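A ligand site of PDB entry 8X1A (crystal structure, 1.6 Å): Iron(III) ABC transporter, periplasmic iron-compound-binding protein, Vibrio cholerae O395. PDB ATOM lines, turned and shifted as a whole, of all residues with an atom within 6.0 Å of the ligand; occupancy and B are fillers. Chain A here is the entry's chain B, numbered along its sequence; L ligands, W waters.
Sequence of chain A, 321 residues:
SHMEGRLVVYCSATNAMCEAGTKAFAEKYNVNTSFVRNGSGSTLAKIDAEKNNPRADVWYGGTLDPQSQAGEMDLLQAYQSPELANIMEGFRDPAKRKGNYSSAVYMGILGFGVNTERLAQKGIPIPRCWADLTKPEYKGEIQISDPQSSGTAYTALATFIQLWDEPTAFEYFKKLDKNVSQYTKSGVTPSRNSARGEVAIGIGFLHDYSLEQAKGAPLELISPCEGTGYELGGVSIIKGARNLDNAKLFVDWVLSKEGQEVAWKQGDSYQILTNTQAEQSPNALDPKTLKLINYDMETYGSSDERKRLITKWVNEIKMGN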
ATOM      1  N   SER A  12      -3.050  13.831  23.783  1.00  0.00           N
ATOM      2  CA  SER A  12      -2.042  13.450  22.785  1.00  0.00           C
ATOM      3  C   SER A  12      -1.737  11.924  22.803  1.00  0.00           C
ATOM      4  O   SER A  12      -0.818  11.456  22.107  1.00  0.00           O
ATOM      5  CB  SER A  12      -0.751  14.276  23.011  1.00  0.00           C
ATOM      6  OG  SER A  12      -1.033  15.673  22.778  1.00  0.00           O
ATOM      7  N   ALA A  13      -2.474  11.169  23.614  1.00  0.00           N
ATOM      8  CA  ALA A  13      -2.435   9.696  23.529  1.00  0.00           C
ATOM      9  C   ALA A  13      -3.236   9.256  22.335  1.00  0.00           C
ATOM     10  O   ALA A  13      -3.675  10.080  21.530  1.00  0.00           O
ATOM     11  CB  ALA A  13      -2.985   9.066  24.802  1.00  0.00           C
ATOM     12  N   THR A  14      -3.439   7.950  22.164  1.00  0.00           N
ATOM     13  CA  THR A  14      -4.329   7.517  21.082  1.00  0.00           C
ATOM     14  C   THR A  14      -5.750   7.951  21.360  1.00  0.00           C
ATOM     15  O   THR A  14      -6.161   8.120  22.495  1.00  0.00           O
ATOM     16  CB  THR A  14      -4.354   5.995  20.886  1.00  0.00           C
ATOM     17  OG1 THR A  14      -4.761   5.374  22.129  1.00  0.00           O
ATOM     18  CG2 THR A  14      -2.976   5.479  20.452  1.00  0.00           C
ATOM     19  N   ARG A  37      -7.818  15.309  20.050  1.00  0.00           N
ATOM     20  CA  ARG A  37      -6.552  14.579  20.050  1.00  0.00           C
ATOM     21  C   ARG A  37      -5.642  15.202  18.997  1.00  0.00           C
ATOM     22  O   ARG A  37      -6.094  15.461  17.896  1.00  0.00           O
ATOM     23  CB  ARG A  37      -6.782  13.097  19.768  1.00  0.00           C
ATOM     24  CG  ARG A  37      -5.577  12.205  20.085  1.00  0.00           C
ATOM     25  CD  ARG A  37      -4.600  12.122  18.897  1.00  0.00           C
ATOM     26  NE  ARG A  37      -3.243  11.938  19.384  1.00  0.00           N
ATOM     27  CZ  ARG A  37      -2.153  12.128  18.645  1.00  0.00           C
ATOM     28  NH1 ARG A  37      -2.268  12.479  17.345  1.00  0.00           N
ATOM     29  NH2 ARG A  37      -0.951  11.951  19.191  1.00  0.00           N
ATOM     30  N   ASN A  38      -4.399  15.511  19.384  1.00  0.00           N
ATOM     31  CA  ASN A  38      -3.430  16.064  18.446  1.00  0.00           C
ATOM     32  C   ASN A  38      -2.039  15.591  18.834  1.00  0.00           C
ATOM     33  O   ASN A  38      -1.818  15.267  20.005  1.00  0.00           O
ATOM     34  CB  ASN A  38      -3.445  17.622  18.482  1.00  0.00           C
ATOM     35  CG  ASN A  38      -4.800  18.210  18.117  1.00  0.00           C
ATOM     36  OD1 ASN A  38      -5.144  18.326  16.955  1.00  0.00           O
ATOM     37  ND2 ASN A  38      -5.562  18.625  19.132  1.00  0.00           N
ATOM     38  N   GLY A  39      -1.102  15.633  17.899  1.00  0.00           N
ATOM     39  CA  GLY A  39       0.273  15.268  18.225  1.00  0.00           C
ATOM     40  C   GLY A  39       0.814  16.129  19.354  1.00  0.00           C
ATOM     41  O   GLY A  39       0.327  17.234  19.593  1.00  0.00           O
ATOM     42  N   SER A  40       1.805  15.592  20.061  1.00  0.00           N
ATOM     43  CA  SER A  40       2.336  16.278  21.240  1.00  0.00           C
ATOM     44  C   SER A  40       2.932  17.656  20.905  1.00  0.00           C
ATOM     45  O   SER A  40       2.741  18.639  21.662  1.00  0.00           O
ATOM     46  CB  SER A  40       3.418  15.404  21.912  1.00  0.00           C
ATOM     47  OG  SER A  40       2.936  14.119  22.275  1.00  0.00           O
ATOM     48  N   GLY A  41       3.655  17.740  19.807  1.00  0.00           N
ATOM     49  CA  GLY A  41       4.236  19.010  19.343  1.00  0.00           C
ATOM     50  C   GLY A  41       3.173  19.954  18.815  1.00  0.00           C
ATOM     51  O   GLY A  41       3.223  21.174  19.061  1.00  0.00           O
ATOM     52  N   GLY A  61      -1.518  12.967  28.127  1.00  0.00           N
ATOM     53  CA  GLY A  61      -0.878  11.989  27.240  1.00  0.00           C
ATOM     54  C   GLY A  61       0.027  12.665  26.232  1.00  0.00           C
ATOM     55  O   GLY A  61       0.213  13.900  26.282  1.00  0.00           O
ATOM     56  N   GLY A  62       0.587  11.856  25.325  1.00  0.00           N
ATOM     57  CA  GLY A  62       1.650  12.364  24.496  1.00  0.00           C
ATOM     58  C   GLY A  62       2.920  12.329  25.322  1.00  0.00           C
ATOM     59  O   GLY A  62       2.903  12.031  26.516  1.00  0.00           O
ATOM     60  N   THR A  63       4.034  12.682  24.689  1.00  0.00           N
ATOM     61  CA  THR A  63       5.321  12.602  25.366  1.00  0.00           C
ATOM     62  C   THR A  63       5.556  13.783  26.281  1.00  0.00           C
ATOM     63  O   THR A  63       4.926  14.831  26.155  1.00  0.00           O
ATOM     64  CB  THR A  63       6.473  12.540  24.344  1.00  0.00           C
ATOM     65  OG1 THR A  63       6.466  13.752  23.577  1.00  0.00           O
ATOM     66  CG2 THR A  63       6.277  11.382  23.368  1.00  0.00           C
ATOM     67  N   TYR A 106       2.586   7.547  32.348  1.00  0.00           N
ATOM     68  CA  TYR A 106       2.913   6.221  31.790  1.00  0.00           C
ATOM     69  C   TYR A 106       4.299   6.275  31.203  1.00  0.00           C
ATOM     70  O   TYR A 106       4.926   7.344  31.183  1.00  0.00           O
ATOM     71  CB  TYR A 106       1.904   5.743  30.737  1.00  0.00           C
ATOM     72  CG  TYR A 106       1.656   6.652  29.535  1.00  0.00           C
ATOM     73  CD1 TYR A 106       2.571   6.747  28.484  1.00  0.00           C
ATOM     74  CD2 TYR A 106       0.416   7.330  29.397  1.00  0.00           C
ATOM     75  CE1 TYR A 106       2.306   7.541  27.341  1.00  0.00           C
ATOM     76  CE2 TYR A 106       0.156   8.135  28.282  1.00  0.00           C
ATOM     77  CZ  TYR A 106       1.087   8.208  27.237  1.00  0.00           C
ATOM     78  OH  TYR A 106       0.810   9.010  26.159  1.00  0.00           O
ATOM     79  N   GLY A 108       6.531   4.582  27.811  1.00  0.00           N
ATOM     80  CA  GLY A 108       6.383   3.857  26.555  1.00  0.00           C
ATOM     81  C   GLY A 108       7.743   3.608  25.919  1.00  0.00           C
ATOM     82  O   GLY A 108       8.601   4.514  25.965  1.00  0.00           O
ATOM     83  N   SER A 145       7.572   9.278  12.249  1.00  0.00           N
ATOM     84  CA  SER A 145       6.941  10.573  12.417  1.00  0.00           C
ATOM     85  C   SER A 145       7.914  11.751  12.344  1.00  0.00           C
ATOM     86  O   SER A 145       9.130  11.567  12.267  1.00  0.00           O
ATOM     87  CB  SER A 145       6.219  10.571  13.756  1.00  0.00           C
ATOM     88  OG  SER A 145       7.049  10.000  14.758  1.00  0.00           O
ATOM     89  N   SER A 149       5.793  18.060  14.819  1.00  0.00           N
ATOM     90  CA  SER A 149       4.436  17.890  15.327  1.00  0.00           C
ATOM     91  C   SER A 149       4.285  16.704  16.300  1.00  0.00           C
ATOM     92  O   SER A 149       3.389  16.693  17.171  1.00  0.00           O
ATOM     93  CB  SER A 149       3.456  17.710  14.161  1.00  0.00           C
ATOM     94  OG  SER A 149       3.973  16.719  13.302  1.00  0.00           O
ATOM     95  N   SER A 150       5.165  15.706  16.173  1.00  0.00           N
ATOM     96  CA  SER A 150       5.041  14.458  16.936  1.00  0.00           C
ATOM     97  C   SER A 150       6.021  14.386  18.104  1.00  0.00           C
ATOM     98  O   SER A 150       7.211  14.672  17.932  1.00  0.00           O
ATOM     99  CB  SER A 150       5.264  13.278  15.989  1.00  0.00           C
ATOM    100  OG  SER A 150       5.588  12.101  16.672  1.00  0.00           O
ATOM    101  N   GLY A 151       5.527  14.019  19.294  1.00  0.00           N
ATOM    102  CA  GLY A 151       6.393  13.748  20.444  1.00  0.00           C
ATOM    103  C   GLY A 151       7.297  12.523  20.207  1.00  0.00           C
ATOM    104  O   GLY A 151       8.477  12.535  20.572  1.00  0.00           O
ATOM    105  N   THR A 152       6.733  11.494  19.576  1.00  0.00           N
ATOM    106  CA  THR A 152       7.426  10.251  19.321  1.00  0.00           C
ATOM    107  C   THR A 152       8.687  10.500  18.526  1.00  0.00           C
ATOM    108  O   THR A 152       9.767   9.961  18.824  1.00  0.00           O
ATOM    109  CB  THR A 152       6.534   9.260  18.528  1.00  0.00           C
ATOM    110  OG1 THR A 152       5.301   9.083  19.245  1.00  0.00           O
ATOM    111  CG2 THR A 152       7.232   7.897  18.353  1.00  0.00           C
ATOM    112  N   ALA A 153       8.564  11.325  17.509  1.00  0.00           N
ATOM    113  CA  ALA A 153       9.668  11.559  16.619  1.00  0.00           C
ATOM    114  C   ALA A 153      10.819  12.267  17.312  1.00  0.00           C
ATOM    115  O   ALA A 153      11.989  12.035  16.978  1.00  0.00           O
ATOM    116  CB  ALA A 153       9.198  12.391  15.411  1.00  0.00           C
ATOM    117  N   LYS A 185       2.639  13.054  10.678  1.00  0.00           N
ATOM    118  CA  LYS A 185       2.440  14.171  11.591  1.00  0.00           C
ATOM    119  C   LYS A 185       2.248  13.693  13.042  1.00  0.00           C
ATOM    120  O   LYS A 185       2.558  14.432  13.957  1.00  0.00           O
ATOM    121  CB  LYS A 185       1.242  15.015  11.138  1.00  0.00           C
ATOM    122  CG  LYS A 185       1.545  15.679   9.800  1.00  0.00           C
ATOM    123  CD  LYS A 185       0.239  16.160   9.130  1.00  0.00           C
ATOM    124  CE  LYS A 185       0.519  16.866   7.778  1.00  0.00           C
ATOM    125  NZ  LYS A 185       1.075  15.961   6.725  1.00  0.00           N
ATOM    126  N   SER A 186       1.711  12.481  13.223  1.00  0.00           N
ATOM    127  CA  SER A 186       1.612  11.902  14.577  1.00  0.00           C
ATOM    128  C   SER A 186       2.381  10.593  14.684  1.00  0.00           C
ATOM    129  O   SER A 186       2.730   9.953  13.683  1.00  0.00           O
ATOM    130  CB  SER A 186       0.154  11.686  14.991  1.00  0.00           C
ATOM    131  OG  SER A 186      -0.453  12.942  15.258  1.00  0.00           O
ATOM    132  N   GLY A 187       2.701  10.216  15.922  1.00  0.00           N
ATOM    133  CA  GLY A 187       3.573   9.092  16.165  1.00  0.00           C
ATOM    134  C   GLY A 187       3.007   7.727  15.877  1.00  0.00           C
ATOM    135  O   GLY A 187       3.774   6.805  15.501  1.00  0.00           O
ATOM    136  N   VAL A 188       1.687   7.577  16.009  1.00  0.00           N
ATOM    137  CA  VAL A 188       1.044   6.260  15.880  1.00  0.00           C
ATOM    138  C   VAL A 188       0.911   5.789  14.453  1.00  0.00           C
ATOM    139  O   VAL A 188       0.794   4.597  14.197  1.00  0.00           O
ATOM    140  CB  VAL A 188      -0.371   6.275  16.542  1.00  0.00           C
ATOM    141  CG1 VAL A 188      -1.378   7.058  15.685  1.00  0.00           C
ATOM    142  CG2 VAL A 188      -0.867   4.877  16.790  1.00  0.00           C
ATOM    143  N   PHE A 205       6.386   3.872  19.323  1.00  0.00           N
ATOM    144  CA  PHE A 205       6.350   3.228  20.626  1.00  0.00           C
ATOM    145  C   PHE A 205       5.734   1.835  20.511  1.00  0.00           C
ATOM    146  O   PHE A 205       4.705   1.618  19.828  1.00  0.00           O
ATOM    147  CB  PHE A 205       5.601   4.117  21.623  1.00  0.00           C
ATOM    148  CG  PHE A 205       6.325   5.408  21.901  1.00  0.00           C
ATOM    149  CD1 PHE A 205       7.621   5.375  22.382  1.00  0.00           C
ATOM    150  CD2 PHE A 205       5.749   6.646  21.623  1.00  0.00           C
ATOM    151  CE1 PHE A 205       8.335   6.578  22.631  1.00  0.00           C
ATOM    152  CE2 PHE A 205       6.432   7.851  21.866  1.00  0.00           C
ATOM    153  CZ  PHE A 205       7.740   7.809  22.381  1.00  0.00           C
ATOM    154  N   HIS A 207       4.134  -0.321  22.372  1.00  0.00           N
ATOM    155  CA  HIS A 207       2.789  -0.775  22.761  1.00  0.00           C
ATOM    156  C   HIS A 207       1.739  -0.557  21.624  1.00  0.00           C
ATOM    157  O   HIS A 207       0.760  -1.319  21.511  1.00  0.00           O
ATOM    158  CB  HIS A 207       2.359  -0.076  24.049  1.00  0.00           C
ATOM    159  CG  HIS A 207       2.417   1.400  23.972  1.00  0.00           C
ATOM    160  ND1 HIS A 207       3.569   2.130  24.230  1.00  0.00           N
ATOM    161  CD2 HIS A 207       1.460   2.310  23.634  1.00  0.00           C
ATOM    162  CE1 HIS A 207       3.318   3.403  24.052  1.00  0.00           C
ATOM    163  NE2 HIS A 207       2.047   3.552  23.672  1.00  0.00           N
ATOM    164  N   ASP A 208       1.930   0.457  20.779  1.00  0.00           N
ATOM    165  CA  ASP A 208       1.001   0.653  19.661  1.00  0.00           C
ATOM    166  C   ASP A 208       1.107  -0.538  18.696  1.00  0.00           C
ATOM    167  O   ASP A 208       0.118  -0.947  18.093  1.00  0.00           O
ATOM    168  CB  ASP A 208       1.271   1.951  18.916  1.00  0.00           C
ATOM    169  CG  ASP A 208       1.042   3.202  19.770  1.00  0.00           C
ATOM    170  OD1 ASP A 208       0.142   3.164  20.653  1.00  0.00           O
ATOM    171  OD2 ASP A 208       1.735   4.201  19.536  1.00  0.00           O
ATOM    172  N   GLU A 231       9.505   7.171  26.263  1.00  0.00           N
ATOM    173  CA  GLU A 231       8.744   8.371  26.647  1.00  0.00           C
ATOM    174  C   GLU A 231       8.251   8.191  28.068  1.00  0.00           C
ATOM    175  O   GLU A 231       8.052   7.068  28.555  1.00  0.00           O
ATOM    176  CB  GLU A 231       7.518   8.607  25.744  1.00  0.00           C
ATOM    177  CG  GLU A 231       6.619   7.355  25.593  1.00  0.00           C
ATOM    178  CD  GLU A 231       5.216   7.627  25.090  1.00  0.00           C
ATOM    179  OE1 GLU A 231       4.851   8.821  24.943  1.00  0.00           O
ATOM    180  OE2 GLU A 231       4.461   6.626  24.834  1.00  0.00           O
ATOM    181  N   GLY A 233       4.663   9.536  29.480  1.00  0.00           N
ATOM    182  CA  GLY A 233       3.453  10.237  29.099  1.00  0.00           C
ATOM    183  C   GLY A 233       3.185  11.317  30.105  1.00  0.00           C
ATOM    184  O   GLY A 233       3.249  11.065  31.309  1.00  0.00           O
ATOM    185  N   SER A 269      -4.465   0.477  25.410  1.00  0.00           N
ATOM    186  CA  SER A 269      -3.213   1.220  25.327  1.00  0.00           C
ATOM    187  C   SER A 269      -2.294   0.659  26.385  1.00  0.00           C
ATOM    188  O   SER A 269      -2.583   0.795  27.565  1.00  0.00           O
ATOM    189  CB  SER A 269      -3.504   2.712  25.516  1.00  0.00           C
ATOM    190  OG  SER A 269      -2.350   3.493  25.305  1.00  0.00           O
ATOM    191  N   GLN A 271       0.879   0.960  27.573  1.00  0.00           N
ATOM    192  CA  GLN A 271       2.047   1.536  28.196  1.00  0.00           C
ATOM    193  C   GLN A 271       2.269   0.961  29.576  1.00  0.00           C
ATOM    194  O   GLN A 271       1.335   0.463  30.245  1.00  0.00           O
ATOM    195  CB  GLN A 271       1.939   3.054  28.308  1.00  0.00           C
ATOM    196  CG  GLN A 271       1.732   3.779  26.975  1.00  0.00           C
ATOM    197  CD  GLN A 271       0.285   4.150  26.736  1.00  0.00           C
ATOM    198  OE1 GLN A 271      -0.626   3.437  27.170  1.00  0.00           O
ATOM    199  NE2 GLN A 271       0.064   5.248  26.010  1.00  0.00           N
HETATM  200  C1  LIG L   1       1.165   6.929  20.705  1.00  0.00           C
HETATM  201  C2  LIG L   1       1.243   6.231  22.030  1.00  0.00           C
HETATM  202  C3  LIG L   1       1.452   7.171  23.167  1.00  0.00           C
HETATM  203  C4  LIG L   1       2.362   8.341  22.901  1.00  0.00           C
HETATM  204  C5  LIG L   1       1.749   9.220  21.800  1.00  0.00           C
HETATM  205  C6  LIG L   1       2.669  10.287  21.245  1.00  0.00           C
HETATM  206  O1  LIG L   1       0.244   6.460  19.786  1.00  0.00           O
HETATM  207  O2  LIG L   1       0.153   5.298  22.268  1.00  0.00           O
HETATM  208  O3  LIG L   1       2.018   6.318  24.157  1.00  0.00           O
HETATM  209  O4  LIG L   1       2.532   9.188  24.039  1.00  0.00           O
HETATM  210  O5  LIG L   1       1.478   8.386  20.654  1.00  0.00           O
HETATM  211  O6  LIG L   1       1.977  10.880  20.143  1.00  0.00           O
HETATM  212  P1  LIG L   1       2.662  11.858  19.088  1.00  0.00           P
HETATM  213  O7  LIG L   1       3.920  11.186  18.607  1.00  0.00           O
HETATM  214  O8  LIG L   1       1.682  12.060  17.966  1.00  0.00           O
HETATM  215  O9  LIG L   1       2.977  13.135  19.797  1.00  0.00           O
HETATM  216  O   HOH W   1      -2.056   5.806  23.987  1.00  0.00           O
HETATM  217  O   HOH W   2       0.473   9.209  18.075  1.00  0.00           O
HETATM  218  O   HOH W   3       3.501   7.142  18.795  1.00  0.00           O
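O of Ser 12 sits close to O6 of the ligand, 3.5 Å away. Merely in contact with the ligand: Val 188 (3.3 Å), Gly 62 (3.3 Å), Ser 186 (3.4 Å), Thr 14 (3.4 Å), Gly 39 (3.5 Å), Thr 63 (3.9 Å) and Phe 205 (3.997 Å). Hydrophobic or aromatic side chains within 4 Å of the ligand: Tyr 106, Val 188, Phe 205 and His 207. Of the 30 residues printed, 19 come within 4 Å of the ligand. Along chain A the residues within 4 Å of the ligand span positions 12 to 271. The nearest printed residue that does not touch the ligand is Ser 269 (4.3 Å).
Water W1 lies within hydrogen-bond range of the side-chain hydroxyl (OG) of Ser 269 (2.7 Å), an oxygen (O2) of the ligand (2.8 Å), the side-chain amide nitrogen (NE2) of Gln 271 (3.0 Å) and the backbone NH (N) of Thr 14 (3.1 Å). Water W3 lies within hydrogen-bond range of OG1 of Thr 152 (2.7 Å), O5 of the ligand (3.0 Å), O of Gly 187 (3.3 Å) and N of Val 188 (3.4 Å).
O3 of the ligand lies within hydrogen-bond range of NE2 of Gln 271 (2.9 Å). O8 of the ligand is in salt-bridge range of NH2 of Arg 37 (2.9 Å). The backbone NH (N) of Gly 187 is in hydrogen-bond range of an oxygen (O8) of the ligand, at 2.9 Å. The side-chain carboxylate of Glu 231 is in hydrogen-bond range of an oxygen (O4) of the ligand (2.5 Å). O4 of the ligand sits at hydrogen-bond distance from OH of Tyr 106, 2.7 Å away. The backbone NH (N) of Ser 40 sits at hydrogen-bond distance from an oxygen (O9) of the ligand, at 2.7 Å. An oxygen (O9) of the ligand sits at hydrogen-bond distance from the backbone NH (N) of Gly 151, at 2.7 Å. The backbone NH of Thr 152 lies within hydrogen-bond range of an oxygen (O7) of the ligand. The side-chain hydroxyl (OG) of Ser 40 is in hydrogen-bond range of an oxygen (O9) of the ligand, at 2.7 Å. An oxygen (O7) of the ligand is in hydrogen-bond range of the side-chain hydroxyl (OG1) of Thr 152 (2.6 Å). An oxygen (O7) of the ligand sits at hydrogen-bond distance from the side-chain hydroxyl (OG) of Ser 150. A ring nitrogen (NE2) of His 207 is in hydrogen-bond range of an oxygen (O3) of the ligand. The side-chain carboxylate of Asp 208 is in hydrogen-bond range of an oxygen (O2) of the ligand.
The side-chain hydroxyl of Ser 12 is in hydrogen-bond range of the backbone carbonyl oxygen of Asn 38, at 2.9 Å. The backbone NH of Ser 40 sits at hydrogen-bond distance from the backbone carbonyl oxygen of Ser 149 (3.5 Å). O of Tyr 106 lies within hydrogen-bond range of N of Gly 233 (2.8 Å). The side-chain hydroxyl of Ser 150 lies within hydrogen-bond range of the side-chain hydroxyl of Ser 145 (3.2 Å). The backbone carbonyl oxygen of Gly 108 sits at hydrogen-bond distance from the backbone NH of Glu 231, at 2.8 Å. OG of Ser 186 sits at hydrogen-bond distance from NH1 of Arg 37, 2.8 Å away. The guanidinium group of Arg 37 is in hydrogen-bond range of the backbone carbonyl oxygen of Ala 13. N of Thr 152 sits at hydrogen-bond distance from OG of Ser 150, 3.2 Å away.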
